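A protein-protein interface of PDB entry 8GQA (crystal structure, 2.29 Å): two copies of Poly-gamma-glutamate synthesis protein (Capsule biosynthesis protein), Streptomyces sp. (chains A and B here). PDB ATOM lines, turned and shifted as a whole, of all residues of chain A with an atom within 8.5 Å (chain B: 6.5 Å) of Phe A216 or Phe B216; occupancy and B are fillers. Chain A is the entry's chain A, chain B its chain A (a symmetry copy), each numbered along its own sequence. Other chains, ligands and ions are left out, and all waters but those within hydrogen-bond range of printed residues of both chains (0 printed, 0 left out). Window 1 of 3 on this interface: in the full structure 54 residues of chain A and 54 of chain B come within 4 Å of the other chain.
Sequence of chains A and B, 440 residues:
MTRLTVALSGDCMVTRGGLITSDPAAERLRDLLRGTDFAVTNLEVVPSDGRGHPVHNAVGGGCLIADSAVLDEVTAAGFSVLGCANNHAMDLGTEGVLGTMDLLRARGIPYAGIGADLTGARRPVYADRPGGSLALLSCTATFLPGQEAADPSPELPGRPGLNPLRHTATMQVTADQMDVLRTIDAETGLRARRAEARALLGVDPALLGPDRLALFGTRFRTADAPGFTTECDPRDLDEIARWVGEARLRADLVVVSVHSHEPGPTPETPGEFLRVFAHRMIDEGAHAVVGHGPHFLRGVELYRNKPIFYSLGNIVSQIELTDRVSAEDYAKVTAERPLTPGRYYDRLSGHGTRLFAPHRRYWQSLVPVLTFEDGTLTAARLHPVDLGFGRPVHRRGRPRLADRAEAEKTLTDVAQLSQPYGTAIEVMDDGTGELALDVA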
ATOM      1  N   MET A 171     -13.987   1.484 -16.008  1.00  0.00           N
ATOM      2  CA  MET A 171     -15.165   0.636 -15.916  1.00  0.00           C
ATOM      3  C   MET A 171     -14.721  -0.802 -15.688  1.00  0.00           C
ATOM      4  O   MET A 171     -13.991  -1.369 -16.509  1.00  0.00           O
ATOM      5  CB  MET A 171     -16.009   0.737 -17.186  1.00  0.00           C
ATOM      6  CG  MET A 171     -16.403   2.151 -17.571  1.00  0.00           C
ATOM      7  SD  MET A 171     -18.017   2.609 -16.914  1.00  0.00           S
ATOM      8  CE  MET A 171     -19.097   1.781 -18.079  1.00  0.00           C
ATOM      9  N   VAL A 173     -15.776  -4.546 -15.781  1.00  0.00           N
ATOM     10  CA  VAL A 173     -16.782  -5.362 -16.441  1.00  0.00           C
ATOM     11  C   VAL A 173     -16.386  -6.825 -16.306  1.00  0.00           C
ATOM     12  O   VAL A 173     -15.215  -7.165 -16.124  1.00  0.00           O
ATOM     13  CB  VAL A 173     -16.957  -4.989 -17.930  1.00  0.00           C
ATOM     14  CG1 VAL A 173     -17.510  -3.578 -18.066  1.00  0.00           C
ATOM     15  CG2 VAL A 173     -15.637  -5.125 -18.673  1.00  0.00           C
ATOM     16  N   VAL A 180     -17.950  -9.065 -25.404  1.00  0.00           N
ATOM     17  CA  VAL A 180     -18.917  -8.406 -26.275  1.00  0.00           C
ATOM     18  C   VAL A 180     -18.388  -7.050 -26.730  1.00  0.00           C
ATOM     19  O   VAL A 180     -18.599  -6.641 -27.877  1.00  0.00           O
ATOM     20  CB  VAL A 180     -20.278  -8.287 -25.564  1.00  0.00           C
ATOM     21  CG1 VAL A 180     -21.251  -7.460 -26.395  1.00  0.00           C
ATOM     22  CG2 VAL A 180     -20.852  -9.669 -25.288  1.00  0.00           C
ATOM     23  N   LEU A 181     -17.675  -6.342 -25.849  1.00  0.00           N
ATOM     24  CA  LEU A 181     -17.114  -5.045 -26.219  1.00  0.00           C
ATOM     25  C   LEU A 181     -16.093  -5.186 -27.342  1.00  0.00           C
ATOM     26  O   LEU A 181     -16.124  -4.434 -28.322  1.00  0.00           O
ATOM     27  CB  LEU A 181     -16.483  -4.375 -24.996  1.00  0.00           C
ATOM     28  CG  LEU A 181     -17.430  -3.909 -23.888  1.00  0.00           C
ATOM     29  CD1 LEU A 181     -16.640  -3.419 -22.686  1.00  0.00           C
ATOM     30  CD2 LEU A 181     -18.365  -2.821 -24.395  1.00  0.00           C
ATOM     31  N   ARG A 182     -15.172  -6.148 -27.213  1.00  0.00           N
ATOM     32  CA  ARG A 182     -14.204  -6.393 -28.279  1.00  0.00           C
ATOM     33  C   ARG A 182     -14.890  -6.914 -29.534  1.00  0.00           C
ATOM     34  O   ARG A 182     -14.453  -6.620 -30.653  1.00  0.00           O
ATOM     35  CB  ARG A 182     -13.130  -7.376 -27.813  1.00  0.00           C
ATOM     36  CG  ARG A 182     -12.580  -7.071 -26.439  1.00  0.00           C
ATOM     37  CD  ARG A 182     -11.633  -8.150 -25.924  1.00  0.00           C
ATOM     38  NE  ARG A 182     -10.240  -7.879 -26.275  1.00  0.00           N
ATOM     39  CZ  ARG A 182      -9.227  -7.902 -25.412  1.00  0.00           C
ATOM     40  NH1 ARG A 182      -7.991  -7.645 -25.825  1.00  0.00           N
ATOM     41  NH2 ARG A 182      -9.448  -8.177 -24.134  1.00  0.00           N
ATOM     42  N   THR A 183     -15.957  -7.698 -29.368  1.00  0.00           N
ATOM     43  CA  THR A 183     -16.731  -8.141 -30.520  1.00  0.00           C
ATOM     44  C   THR A 183     -17.331  -6.950 -31.256  1.00  0.00           C
ATOM     45  O   THR A 183     -17.242  -6.855 -32.486  1.00  0.00           O
ATOM     46  CB  THR A 183     -17.823  -9.113 -30.073  1.00  0.00           C
ATOM     47  OG1 THR A 183     -17.221 -10.286 -29.517  1.00  0.00           O
ATOM     48  CG2 THR A 183     -18.700  -9.510 -31.247  1.00  0.00           C
ATOM     49  N   ILE A 184     -17.937  -6.021 -30.511  1.00  0.00           N
ATOM     50  CA  ILE A 184     -18.481  -4.810 -31.119  1.00  0.00           C
ATOM     51  C   ILE A 184     -17.379  -4.019 -31.807  1.00  0.00           C
ATOM     52  O   ILE A 184     -17.574  -3.471 -32.899  1.00  0.00           O
ATOM     53  CB  ILE A 184     -19.209  -3.964 -30.056  1.00  0.00           C
ATOM     54  CG1 ILE A 184     -20.438  -4.709 -29.533  1.00  0.00           C
ATOM     55  CG2 ILE A 184     -19.606  -2.606 -30.623  1.00  0.00           C
ATOM     56  CD1 ILE A 184     -21.114  -4.021 -28.372  1.00  0.00           C
ATOM     57  N   ASP A 185     -16.198  -3.958 -31.189  1.00  0.00           N
ATOM     58  CA  ASP A 185     -15.075  -3.242 -31.787  1.00  0.00           C
ATOM     59  C   ASP A 185     -14.707  -3.829 -33.144  1.00  0.00           C
ATOM     60  O   ASP A 185     -14.495  -3.095 -34.116  1.00  0.00           O
ATOM     61  CB  ASP A 185     -13.876  -3.277 -30.839  1.00  0.00           C
ATOM     62  CG  ASP A 185     -12.646  -2.616 -31.426  1.00  0.00           C
ATOM     63  OD1 ASP A 185     -12.731  -1.430 -31.806  1.00  0.00           O
ATOM     64  OD2 ASP A 185     -11.593  -3.284 -31.507  1.00  0.00           O
ATOM     65  N   ALA A 186     -14.641  -5.158 -33.234  1.00  0.00           N
ATOM     66  CA  ALA A 186     -14.230  -5.797 -34.479  1.00  0.00           C
ATOM     67  C   ALA A 186     -15.343  -5.757 -35.519  1.00  0.00           C
ATOM     68  O   ALA A 186     -15.105  -5.425 -36.686  1.00  0.00           O
ATOM     69  CB  ALA A 186     -13.798  -7.238 -34.209  1.00  0.00           C
ATOM     70  N   THR A 188     -18.097  -3.884 -35.937  1.00  0.00           N
ATOM     71  CA  THR A 188     -18.576  -2.619 -36.485  1.00  0.00           C
ATOM     72  C   THR A 188     -17.634  -2.049 -37.535  1.00  0.00           C
ATOM     73  O   THR A 188     -18.045  -1.183 -38.315  1.00  0.00           O
ATOM     74  CB  THR A 188     -18.771  -1.587 -35.372  1.00  0.00           C
ATOM     75  OG1 THR A 188     -17.555  -1.449 -34.627  1.00  0.00           O
ATOM     76  CG2 THR A 188     -19.901  -2.003 -34.441  1.00  0.00           C
ATOM     77  N   LEU A 190     -14.764  -0.697 -36.353  1.00  0.00           N
ATOM     78  CA  LEU A 190     -13.991   0.272 -35.581  1.00  0.00           C
ATOM     79  C   LEU A 190     -12.531  -0.144 -35.472  1.00  0.00           C
ATOM     80  O   LEU A 190     -11.629   0.693 -35.601  1.00  0.00           O
ATOM     81  CB  LEU A 190     -14.605   0.438 -34.191  1.00  0.00           C
ATOM     82  CG  LEU A 190     -13.954   1.484 -33.284  1.00  0.00           C
ATOM     83  CD1 LEU A 190     -14.199   2.882 -33.825  1.00  0.00           C
ATOM     84  CD2 LEU A 190     -14.467   1.356 -31.857  1.00  0.00           C
ATOM     85  N   ARG A 191     -12.279  -1.433 -35.227  1.00  0.00           N
ATOM     86  CA  ARG A 191     -10.905  -1.916 -35.139  1.00  0.00           C
ATOM     87  C   ARG A 191     -10.156  -1.717 -36.449  1.00  0.00           C
ATOM     88  O   ARG A 191      -8.939  -1.498 -36.442  1.00  0.00           O
ATOM     89  CB  ARG A 191     -10.894  -3.393 -34.740  1.00  0.00           C
ATOM     90  CG  ARG A 191      -9.531  -3.915 -34.317  1.00  0.00           C
ATOM     91  CD  ARG A 191      -9.596  -5.387 -33.939  1.00  0.00           C
ATOM     92  NE  ARG A 191      -9.740  -6.247 -35.110  1.00  0.00           N
ATOM     93  CZ  ARG A 191      -9.902  -7.566 -35.054  1.00  0.00           C
ATOM     94  NH1 ARG A 191      -9.942  -8.182 -33.880  1.00  0.00           N
ATOM     95  NH2 ARG A 191     -10.025  -8.268 -36.171  1.00  0.00           N
ATOM     96  N   ARG A 194      -8.318   1.714 -36.917  1.00  0.00           N
ATOM     97  CA  ARG A 194      -7.081   1.936 -36.182  1.00  0.00           C
ATOM     98  C   ARG A 194      -5.887   1.267 -36.850  1.00  0.00           C
ATOM     99  O   ARG A 194      -4.809   1.203 -36.251  1.00  0.00           O
ATOM    100  CB  ARG A 194      -7.218   1.434 -34.743  1.00  0.00           C
ATOM    101  CG  ARG A 194      -8.371   2.049 -33.970  1.00  0.00           C
ATOM    102  CD  ARG A 194      -8.233   1.785 -32.477  1.00  0.00           C
ATOM    103  NE  ARG A 194      -8.156   0.358 -32.175  1.00  0.00           N
ATOM    104  CZ  ARG A 194      -9.212  -0.413 -31.936  1.00  0.00           C
ATOM    105  NH1 ARG A 194     -10.433   0.104 -31.963  1.00  0.00           N
ATOM    106  NH2 ARG A 194      -9.047  -1.701 -31.670  1.00  0.00           N
ATOM    107  N   ALA A 206      -5.462   0.196 -28.357  1.00  0.00           N
ATOM    108  CA  ALA A 206      -6.658  -0.216 -27.637  1.00  0.00           C
ATOM    109  C   ALA A 206      -6.441  -1.443 -26.762  1.00  0.00           C
ATOM    110  O   ALA A 206      -7.321  -1.772 -25.960  1.00  0.00           O
ATOM    111  CB  ALA A 206      -7.800  -0.494 -28.623  1.00  0.00           C
ATOM    112  N   LEU A 213      -8.166  -2.436 -21.430  1.00  0.00           N
ATOM    113  CA  LEU A 213      -8.715  -2.183 -22.756  1.00  0.00           C
ATOM    114  C   LEU A 213      -9.255  -0.761 -22.827  1.00  0.00           C
ATOM    115  O   LEU A 213      -9.946  -0.312 -21.909  1.00  0.00           O
ATOM    116  CB  LEU A 213      -9.827  -3.177 -23.100  1.00  0.00           C
ATOM    117  CG  LEU A 213      -9.753  -3.857 -24.465  1.00  0.00           C
ATOM    118  CD1 LEU A 213      -8.419  -4.521 -24.744  1.00  0.00           C
ATOM    119  CD2 LEU A 213     -10.862  -4.861 -24.544  1.00  0.00           C
ATOM    120  N   ALA A 214      -8.961  -0.075 -23.934  1.00  0.00           N
ATOM    121  CA  ALA A 214      -9.372   1.311 -24.158  1.00  0.00           C
ATOM    122  C   ALA A 214     -10.205   1.391 -25.435  1.00  0.00           C
ATOM    123  O   ALA A 214      -9.659   1.442 -26.540  1.00  0.00           O
ATOM    124  CB  ALA A 214      -8.161   2.237 -24.245  1.00  0.00           C
ATOM    125  N   LEU A 215     -11.527   1.418 -25.278  1.00  0.00           N
ATOM    126  CA  LEU A 215     -12.454   1.603 -26.384  1.00  0.00           C
ATOM    127  C   LEU A 215     -13.308   2.839 -26.136  1.00  0.00           C
ATOM    128  O   LEU A 215     -13.631   3.169 -24.992  1.00  0.00           O
ATOM    129  CB  LEU A 215     -13.375   0.385 -26.579  1.00  0.00           C
ATOM    130  CG  LEU A 215     -12.789  -1.000 -26.869  1.00  0.00           C
ATOM    131  CD1 LEU A 215     -11.701  -0.929 -27.933  1.00  0.00           C
ATOM    132  CD2 LEU A 215     -12.284  -1.666 -25.600  1.00  0.00           C
ATOM    133  N   PHE A 216     -13.671   3.516 -27.229  1.00  0.00           N
ATOM    134  CA  PHE A 216     -14.584   4.660 -27.196  1.00  0.00           C
ATOM    135  C   PHE A 216     -14.099   5.754 -26.247  1.00  0.00           C
ATOM    136  O   PHE A 216     -14.905   6.438 -25.610  1.00  0.00           O
ATOM    137  CB  PHE A 216     -16.006   4.227 -26.821  1.00  0.00           C
ATOM    138  CG  PHE A 216     -16.334   2.811 -27.209  1.00  0.00           C
ATOM    139  CD1 PHE A 216     -16.331   2.421 -28.538  1.00  0.00           C
ATOM    140  CD2 PHE A 216     -16.642   1.870 -26.241  1.00  0.00           C
ATOM    141  CE1 PHE A 216     -16.631   1.120 -28.894  1.00  0.00           C
ATOM    142  CE2 PHE A 216     -16.944   0.568 -26.590  1.00  0.00           C
ATOM    143  CZ  PHE A 216     -16.939   0.193 -27.919  1.00  0.00           C
ATOM    144  N   GLY A 217     -12.785   5.930 -26.146  1.00  0.00           N
ATOM    145  CA  GLY A 217     -12.238   6.921 -25.234  1.00  0.00           C
ATOM    146  C   GLY A 217     -12.554   6.653 -23.781  1.00  0.00           C
ATOM    147  O   GLY A 217     -12.720   7.597 -23.002  1.00  0.00           O
ATOM    148  N   THR A 218     -12.651   5.382 -23.394  1.00  0.00           N
ATOM    149  CA  THR A 218     -12.958   4.998 -22.026  1.00  0.00           C
ATOM    150  C   THR A 218     -12.160   3.750 -21.676  1.00  0.00           C
ATOM    151  O   THR A 218     -11.890   2.907 -22.535  1.00  0.00           O
ATOM    152  CB  THR A 218     -14.461   4.737 -21.833  1.00  0.00           C
ATOM    153  OG1 THR A 218     -15.212   5.795 -22.443  1.00  0.00           O
ATOM    154  CG2 THR A 218     -14.813   4.667 -20.354  1.00  0.00           C
ATOM    155  N   ARG A 219     -11.780   3.643 -20.406  1.00  0.00           N
ATOM    156  CA  ARG A 219     -11.000   2.514 -19.923  1.00  0.00           C
ATOM    157  C   ARG A 219     -11.926   1.407 -19.432  1.00  0.00           C
ATOM    158  O   ARG A 219     -12.867   1.664 -18.676  1.00  0.00           O
ATOM    159  CB  ARG A 219     -10.056   2.951 -18.802  1.00  0.00           C
ATOM    160  CG  ARG A 219      -8.731   3.508 -19.295  1.00  0.00           C
ATOM    161  CD  ARG A 219      -8.139   4.497 -18.304  1.00  0.00           C
ATOM    162  NE  ARG A 219      -6.724   4.750 -18.564  1.00  0.00           N
ATOM    163  CZ  ARG A 219      -6.270   5.556 -19.518  1.00  0.00           C
ATOM    164  NH1 ARG A 219      -7.119   6.198 -20.311  1.00  0.00           N
ATOM    165  NH2 ARG A 219      -4.965   5.724 -19.681  1.00  0.00           N
ATOM    166  N   PHE A 220     -11.654   0.180 -19.870  1.00  0.00           N
ATOM    167  CA  PHE A 220     -12.383  -1.002 -19.433  1.00  0.00           C
ATOM    168  C   PHE A 220     -11.403  -2.006 -18.846  1.00  0.00           C
ATOM    169  O   PHE A 220     -10.284  -2.158 -19.345  1.00  0.00           O
ATOM    170  CB  PHE A 220     -13.157  -1.644 -20.592  1.00  0.00           C
ATOM    171  CG  PHE A 220     -14.331  -0.835 -21.067  1.00  0.00           C
ATOM    172  CD1 PHE A 220     -15.553  -0.912 -20.417  1.00  0.00           C
ATOM    173  CD2 PHE A 220     -14.218  -0.005 -22.171  1.00  0.00           C
ATOM    174  CE1 PHE A 220     -16.636  -0.172 -20.856  1.00  0.00           C
ATOM    175  CE2 PHE A 220     -15.298   0.737 -22.614  1.00  0.00           C
ATOM    176  CZ  PHE A 220     -16.509   0.653 -21.955  1.00  0.00           C
ATOM    177  N   PHE A 228     -17.170   0.681 -10.799  1.00  0.00           N
ATOM    178  CA  PHE A 228     -16.693   1.965 -11.303  1.00  0.00           C
ATOM    179  C   PHE A 228     -15.652   2.518 -10.341  1.00  0.00           C
ATOM    180  O   PHE A 228     -15.930   2.675  -9.149  1.00  0.00           O
ATOM    181  CB  PHE A 228     -17.855   2.950 -11.467  1.00  0.00           C
ATOM    182  CG  PHE A 228     -17.495   4.195 -12.222  1.00  0.00           C
ATOM    183  CD1 PHE A 228     -17.607   4.239 -13.601  1.00  0.00           C
ATOM    184  CD2 PHE A 228     -17.051   5.322 -11.553  1.00  0.00           C
ATOM    185  CE1 PHE A 228     -17.278   5.384 -14.300  1.00  0.00           C
ATOM    186  CE2 PHE A 228     -16.720   6.470 -12.245  1.00  0.00           C
ATOM    187  CZ  PHE A 228     -16.835   6.501 -13.621  1.00  0.00           C
ATOM    188  N   MET B 171     -21.935   4.126 -34.273  1.00  0.00           N
ATOM    189  CA  MET B 171     -21.730   2.686 -34.273  1.00  0.00           C
ATOM    190  C   MET B 171     -23.079   1.996 -34.415  1.00  0.00           C
ATOM    191  O   MET B 171     -23.970   2.186 -33.579  1.00  0.00           O
ATOM    192  CB  MET B 171     -21.034   2.235 -32.989  1.00  0.00           C
ATOM    193  CG  MET B 171     -19.733   2.955 -32.690  1.00  0.00           C
ATOM    194  SD  MET B 171     -18.303   2.066 -33.330  1.00  0.00           S
ATOM    195  CE  MET B 171     -18.115   0.797 -32.080  1.00  0.00           C
ATOM    196  N   LEU B 181     -24.720  -3.262 -23.817  1.00  0.00           N
ATOM    197  CA  LEU B 181     -24.165  -1.937 -23.554  1.00  0.00           C
ATOM    198  C   LEU B 181     -24.942  -1.223 -22.453  1.00  0.00           C
ATOM    199  O   LEU B 181     -24.351  -0.658 -21.526  1.00  0.00           O
ATOM    200  CB  LEU B 181     -24.156  -1.104 -24.837  1.00  0.00           C
ATOM    201  CG  LEU B 181     -23.196  -1.539 -25.946  1.00  0.00           C
ATOM    202  CD1 LEU B 181     -23.427  -0.714 -27.202  1.00  0.00           C
ATOM    203  CD2 LEU B 181     -21.750  -1.424 -25.488  1.00  0.00           C
ATOM    204  N   ILE B 184     -24.171  -2.910 -19.182  1.00  0.00           N
ATOM    205  CA  ILE B 184     -22.904  -2.423 -18.643  1.00  0.00           C
ATOM    206  C   ILE B 184     -23.080  -1.036 -18.043  1.00  0.00           C
ATOM    207  O   ILE B 184     -22.519  -0.723 -16.986  1.00  0.00           O
ATOM    208  CB  ILE B 184     -21.822  -2.435 -19.740  1.00  0.00           C
ATOM    209  CG1 ILE B 184     -21.520  -3.870 -20.174  1.00  0.00           C
ATOM    210  CG2 ILE B 184     -20.553  -1.742 -19.255  1.00  0.00           C
ATOM    211  CD1 ILE B 184     -20.590  -3.960 -21.359  1.00  0.00           C
ATOM    212  N   ASP B 185     -23.874  -0.186 -18.698  1.00  0.00           N
ATOM    213  CA  ASP B 185     -24.120   1.157 -18.183  1.00  0.00           C
ATOM    214  C   ASP B 185     -24.759   1.109 -16.800  1.00  0.00           C
ATOM    215  O   ASP B 185     -24.350   1.836 -15.887  1.00  0.00           O
ATOM    216  CB  ASP B 185     -25.006   1.931 -19.161  1.00  0.00           C
ATOM    217  CG  ASP B 185     -25.366   3.313 -18.657  1.00  0.00           C
ATOM    218  OD1 ASP B 185     -24.443   4.098 -18.357  1.00  0.00           O
ATOM    219  OD2 ASP B 185     -26.575   3.614 -18.562  1.00  0.00           O
ATOM    220  N   THR B 188     -22.365  -1.176 -13.912  1.00  0.00           N
ATOM    221  CA  THR B 188     -21.106  -0.609 -13.439  1.00  0.00           C
ATOM    222  C   THR B 188     -21.319   0.534 -12.458  1.00  0.00           C
ATOM    223  O   THR B 188     -20.388   0.891 -11.728  1.00  0.00           O
ATOM    224  CB  THR B 188     -20.261  -0.113 -14.614  1.00  0.00           C
ATOM    225  OG1 THR B 188     -21.027   0.807 -15.402  1.00  0.00           O
ATOM    226  CG2 THR B 188     -19.803  -1.277 -15.481  1.00  0.00           C
ATOM    227  N   LEU B 190     -22.372   3.453 -13.813  1.00  0.00           N
ATOM    228  CA  LEU B 190     -22.233   4.626 -14.672  1.00  0.00           C
ATOM    229  C   LEU B 190     -23.549   5.381 -14.795  1.00  0.00           C
ATOM    230  O   LEU B 190     -23.569   6.617 -14.749  1.00  0.00           O
ATOM    231  CB  LEU B 190     -21.729   4.204 -16.052  1.00  0.00           C
ATOM    232  CG  LEU B 190     -21.455   5.332 -17.047  1.00  0.00           C
ATOM    233  CD1 LEU B 190     -20.263   6.159 -16.596  1.00  0.00           C
ATOM    234  CD2 LEU B 190     -21.232   4.777 -18.446  1.00  0.00           C
ATOM    235  N   ALA B 214     -26.313   7.207 -26.409  1.00  0.00           N
ATOM    236  CA  ALA B 214     -25.024   7.885 -26.269  1.00  0.00           C
ATOM    237  C   ALA B 214     -24.351   7.428 -24.977  1.00  0.00           C
ATOM    238  O   ALA B 214     -24.661   7.932 -23.894  1.00  0.00           O
ATOM    239  CB  ALA B 214     -25.195   9.402 -26.281  1.00  0.00           C
ATOM    240  N   LEU B 215     -23.418   6.485 -25.097  1.00  0.00           N
ATOM    241  CA  LEU B 215     -22.611   6.021 -23.979  1.00  0.00           C
ATOM    242  C   LEU B 215     -21.136   6.244 -24.286  1.00  0.00           C
ATOM    243  O   LEU B 215     -20.708   6.161 -25.440  1.00  0.00           O
ATOM    244  CB  LEU B 215     -22.842   4.531 -23.675  1.00  0.00           C
ATOM    245  CG  LEU B 215     -24.237   4.015 -23.308  1.00  0.00           C
ATOM    246  CD1 LEU B 215     -24.909   4.919 -22.283  1.00  0.00           C
ATOM    247  CD2 LEU B 215     -25.104   3.831 -24.542  1.00  0.00           C
ATOM    248  N   PHE B 216     -20.365   6.526 -23.233  1.00  0.00           N
ATOM    249  CA  PHE B 216     -18.909   6.658 -23.317  1.00  0.00           C
ATOM    250  C   PHE B 216     -18.487   7.697 -24.352  1.00  0.00           C
ATOM    251  O   PHE B 216     -17.454   7.547 -25.010  1.00  0.00           O
ATOM    252  CB  PHE B 216     -18.245   5.309 -23.619  1.00  0.00           C
ATOM    253  CG  PHE B 216     -19.025   4.122 -23.127  1.00  0.00           C
ATOM    254  CD1 PHE B 216     -19.269   3.945 -21.774  1.00  0.00           C
ATOM    255  CD2 PHE B 216     -19.516   3.183 -24.019  1.00  0.00           C
ATOM    256  CE1 PHE B 216     -19.987   2.854 -21.322  1.00  0.00           C
ATOM    257  CE2 PHE B 216     -20.234   2.090 -23.572  1.00  0.00           C
ATOM    258  CZ  PHE B 216     -20.469   1.925 -22.222  1.00  0.00           C
ATOM    259  N   GLY B 217     -19.275   8.758 -24.504  1.00  0.00           N
ATOM    260  CA  GLY B 217     -18.968   9.773 -25.497  1.00  0.00           C
ATOM    261  C   GLY B 217     -18.984   9.261 -26.919  1.00  0.00           C
ATOM    262  O   GLY B 217     -18.212   9.742 -27.755  1.00  0.00           O
ATOM    263  N   THR B 218     -19.842   8.287 -27.214  1.00  0.00           N
ATOM    264  CA  THR B 218     -19.945   7.707 -28.543  1.00  0.00           C
ATOM    265  C   THR B 218     -21.406   7.395 -28.830  1.00  0.00           C
ATOM    266  O   THR B 218     -22.176   7.065 -27.924  1.00  0.00           O
ATOM    267  CB  THR B 218     -19.095   6.432 -28.673  1.00  0.00           C
ATOM    268  OG1 THR B 218     -17.795   6.665 -28.116  1.00  0.00           O
ATOM    269  CG2 THR B 218     -18.944   6.029 -30.134  1.00  0.00           C
ATOM    270  N   PHE B 220     -24.379   5.168 -30.401  1.00  0.00           N
ATOM    271  CA  PHE B 220     -24.736   3.797 -30.734  1.00  0.00           C
ATOM    272  C   PHE B 220     -26.156   3.768 -31.280  1.00  0.00           C
ATOM    273  O   PHE B 220     -27.028   4.502 -30.805  1.00  0.00           O
ATOM    274  CB  PHE B 220     -24.628   2.875 -29.513  1.00  0.00           C
ATOM    275  CG  PHE B 220     -23.216   2.622 -29.060  1.00  0.00           C
ATOM    276  CD1 PHE B 220     -22.444   1.645 -29.667  1.00  0.00           C
ATOM    277  CD2 PHE B 220     -22.666   3.352 -28.019  1.00  0.00           C
ATOM    278  CE1 PHE B 220     -21.146   1.408 -29.249  1.00  0.00           C
ATOM    279  CE2 PHE B 220     -21.370   3.119 -27.597  1.00  0.00           C
ATOM    280  CZ  PHE B 220     -20.609   2.145 -28.213  1.00  0.00           C
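O of Phe A216 sits close to O of Phe B216, 2.8 Å away. The backbone carbonyl oxygen (O) of Thr B188 lies close to the backbone NH (N) of Phe A228.
N of Met A171 lies within hydrogen-bond range of O of Arg A219 (2.9 Å). O of Phe A216 sits at hydrogen-bond distance from OG1 of Thr A218. The backbone NH (N) of Leu B190 sits at hydrogen-bond distance from the side-chain hydroxyl (OG1) of Thr B188. The side-chain hydroxyl (OG1) of Thr B188 is in hydrogen-bond range of the backbone carbonyl oxygen (O) of Ile B184, 2.7 Å away. The backbone NH (N) of Leu A190 lies within hydrogen-bond range of the backbone carbonyl oxygen (O) of Asp A185 (3.3 Å). OG1 of Thr A188 is in hydrogen-bond range of N of Leu A190, 3.4 Å away.
CE of Met A171 touches OG1 of Thr B188, 3.4 Å away. Met A171 touches Leu B190. CE of Met A171 touches CE1 of Phe B216, at 3.5 Å. Ile B184 touches Val A173 (CG2 to CG1, 3.7 Å). Leu A181 touches Ile B184. Met B171 touches Ile A184. Leu A190 touches Met B171. CE of Met B171 touches CE1 of Phe A216 (3.5 Å). CB of Phe A216 touches OG1 of Thr B218, 3.3 Å away. CE1 of Phe A228 touches CD1 of Leu B190 (3.8 Å).
Of the printed residues of chain B, Phe A216 touches Met B171, Phe B216 and Thr B218. Phe A220 touches none of the printed residues of chain B. Of the printed residues of chain A, Leu B190 touches Met A171 and Phe A228. Printed residues of chain A within 4 Å of Phe B216: Met A171 (3.5 Å), Phe A216 (2.8 Å) and Thr A218 (3.3 Å). No residue of chain A comes within 4 Å of Gly B217. Of the printed residues of chain A, Thr B218 touches Phe A216. The nearest printed residue of chain B that does not touch Ile A184 is Phe B220 (4.5 Å).
Hydrophobic or aromatic side chains of chain A within 4 Å of the printed part of chain B: Met A171, Val A173, Leu A181, Ile A184, Leu A190, Phe A216 and Phe A228. Among the printed residues, 17 pairs touch across the chains.
Met A171 touches Thr B188, and with the chains exchanged Thr A188 touches Met B171. Leu A181 touches its own counterpart, Leu B181. Leu A181 touches Ile B184, and with the chains exchanged Ile A184 touches Leu B181. Phe A216 touches its own counterpart, Phe B216. Of the 17 pairs that touch across the chains among the printed residues, 14 have their exchanged pair printed and touching as well.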
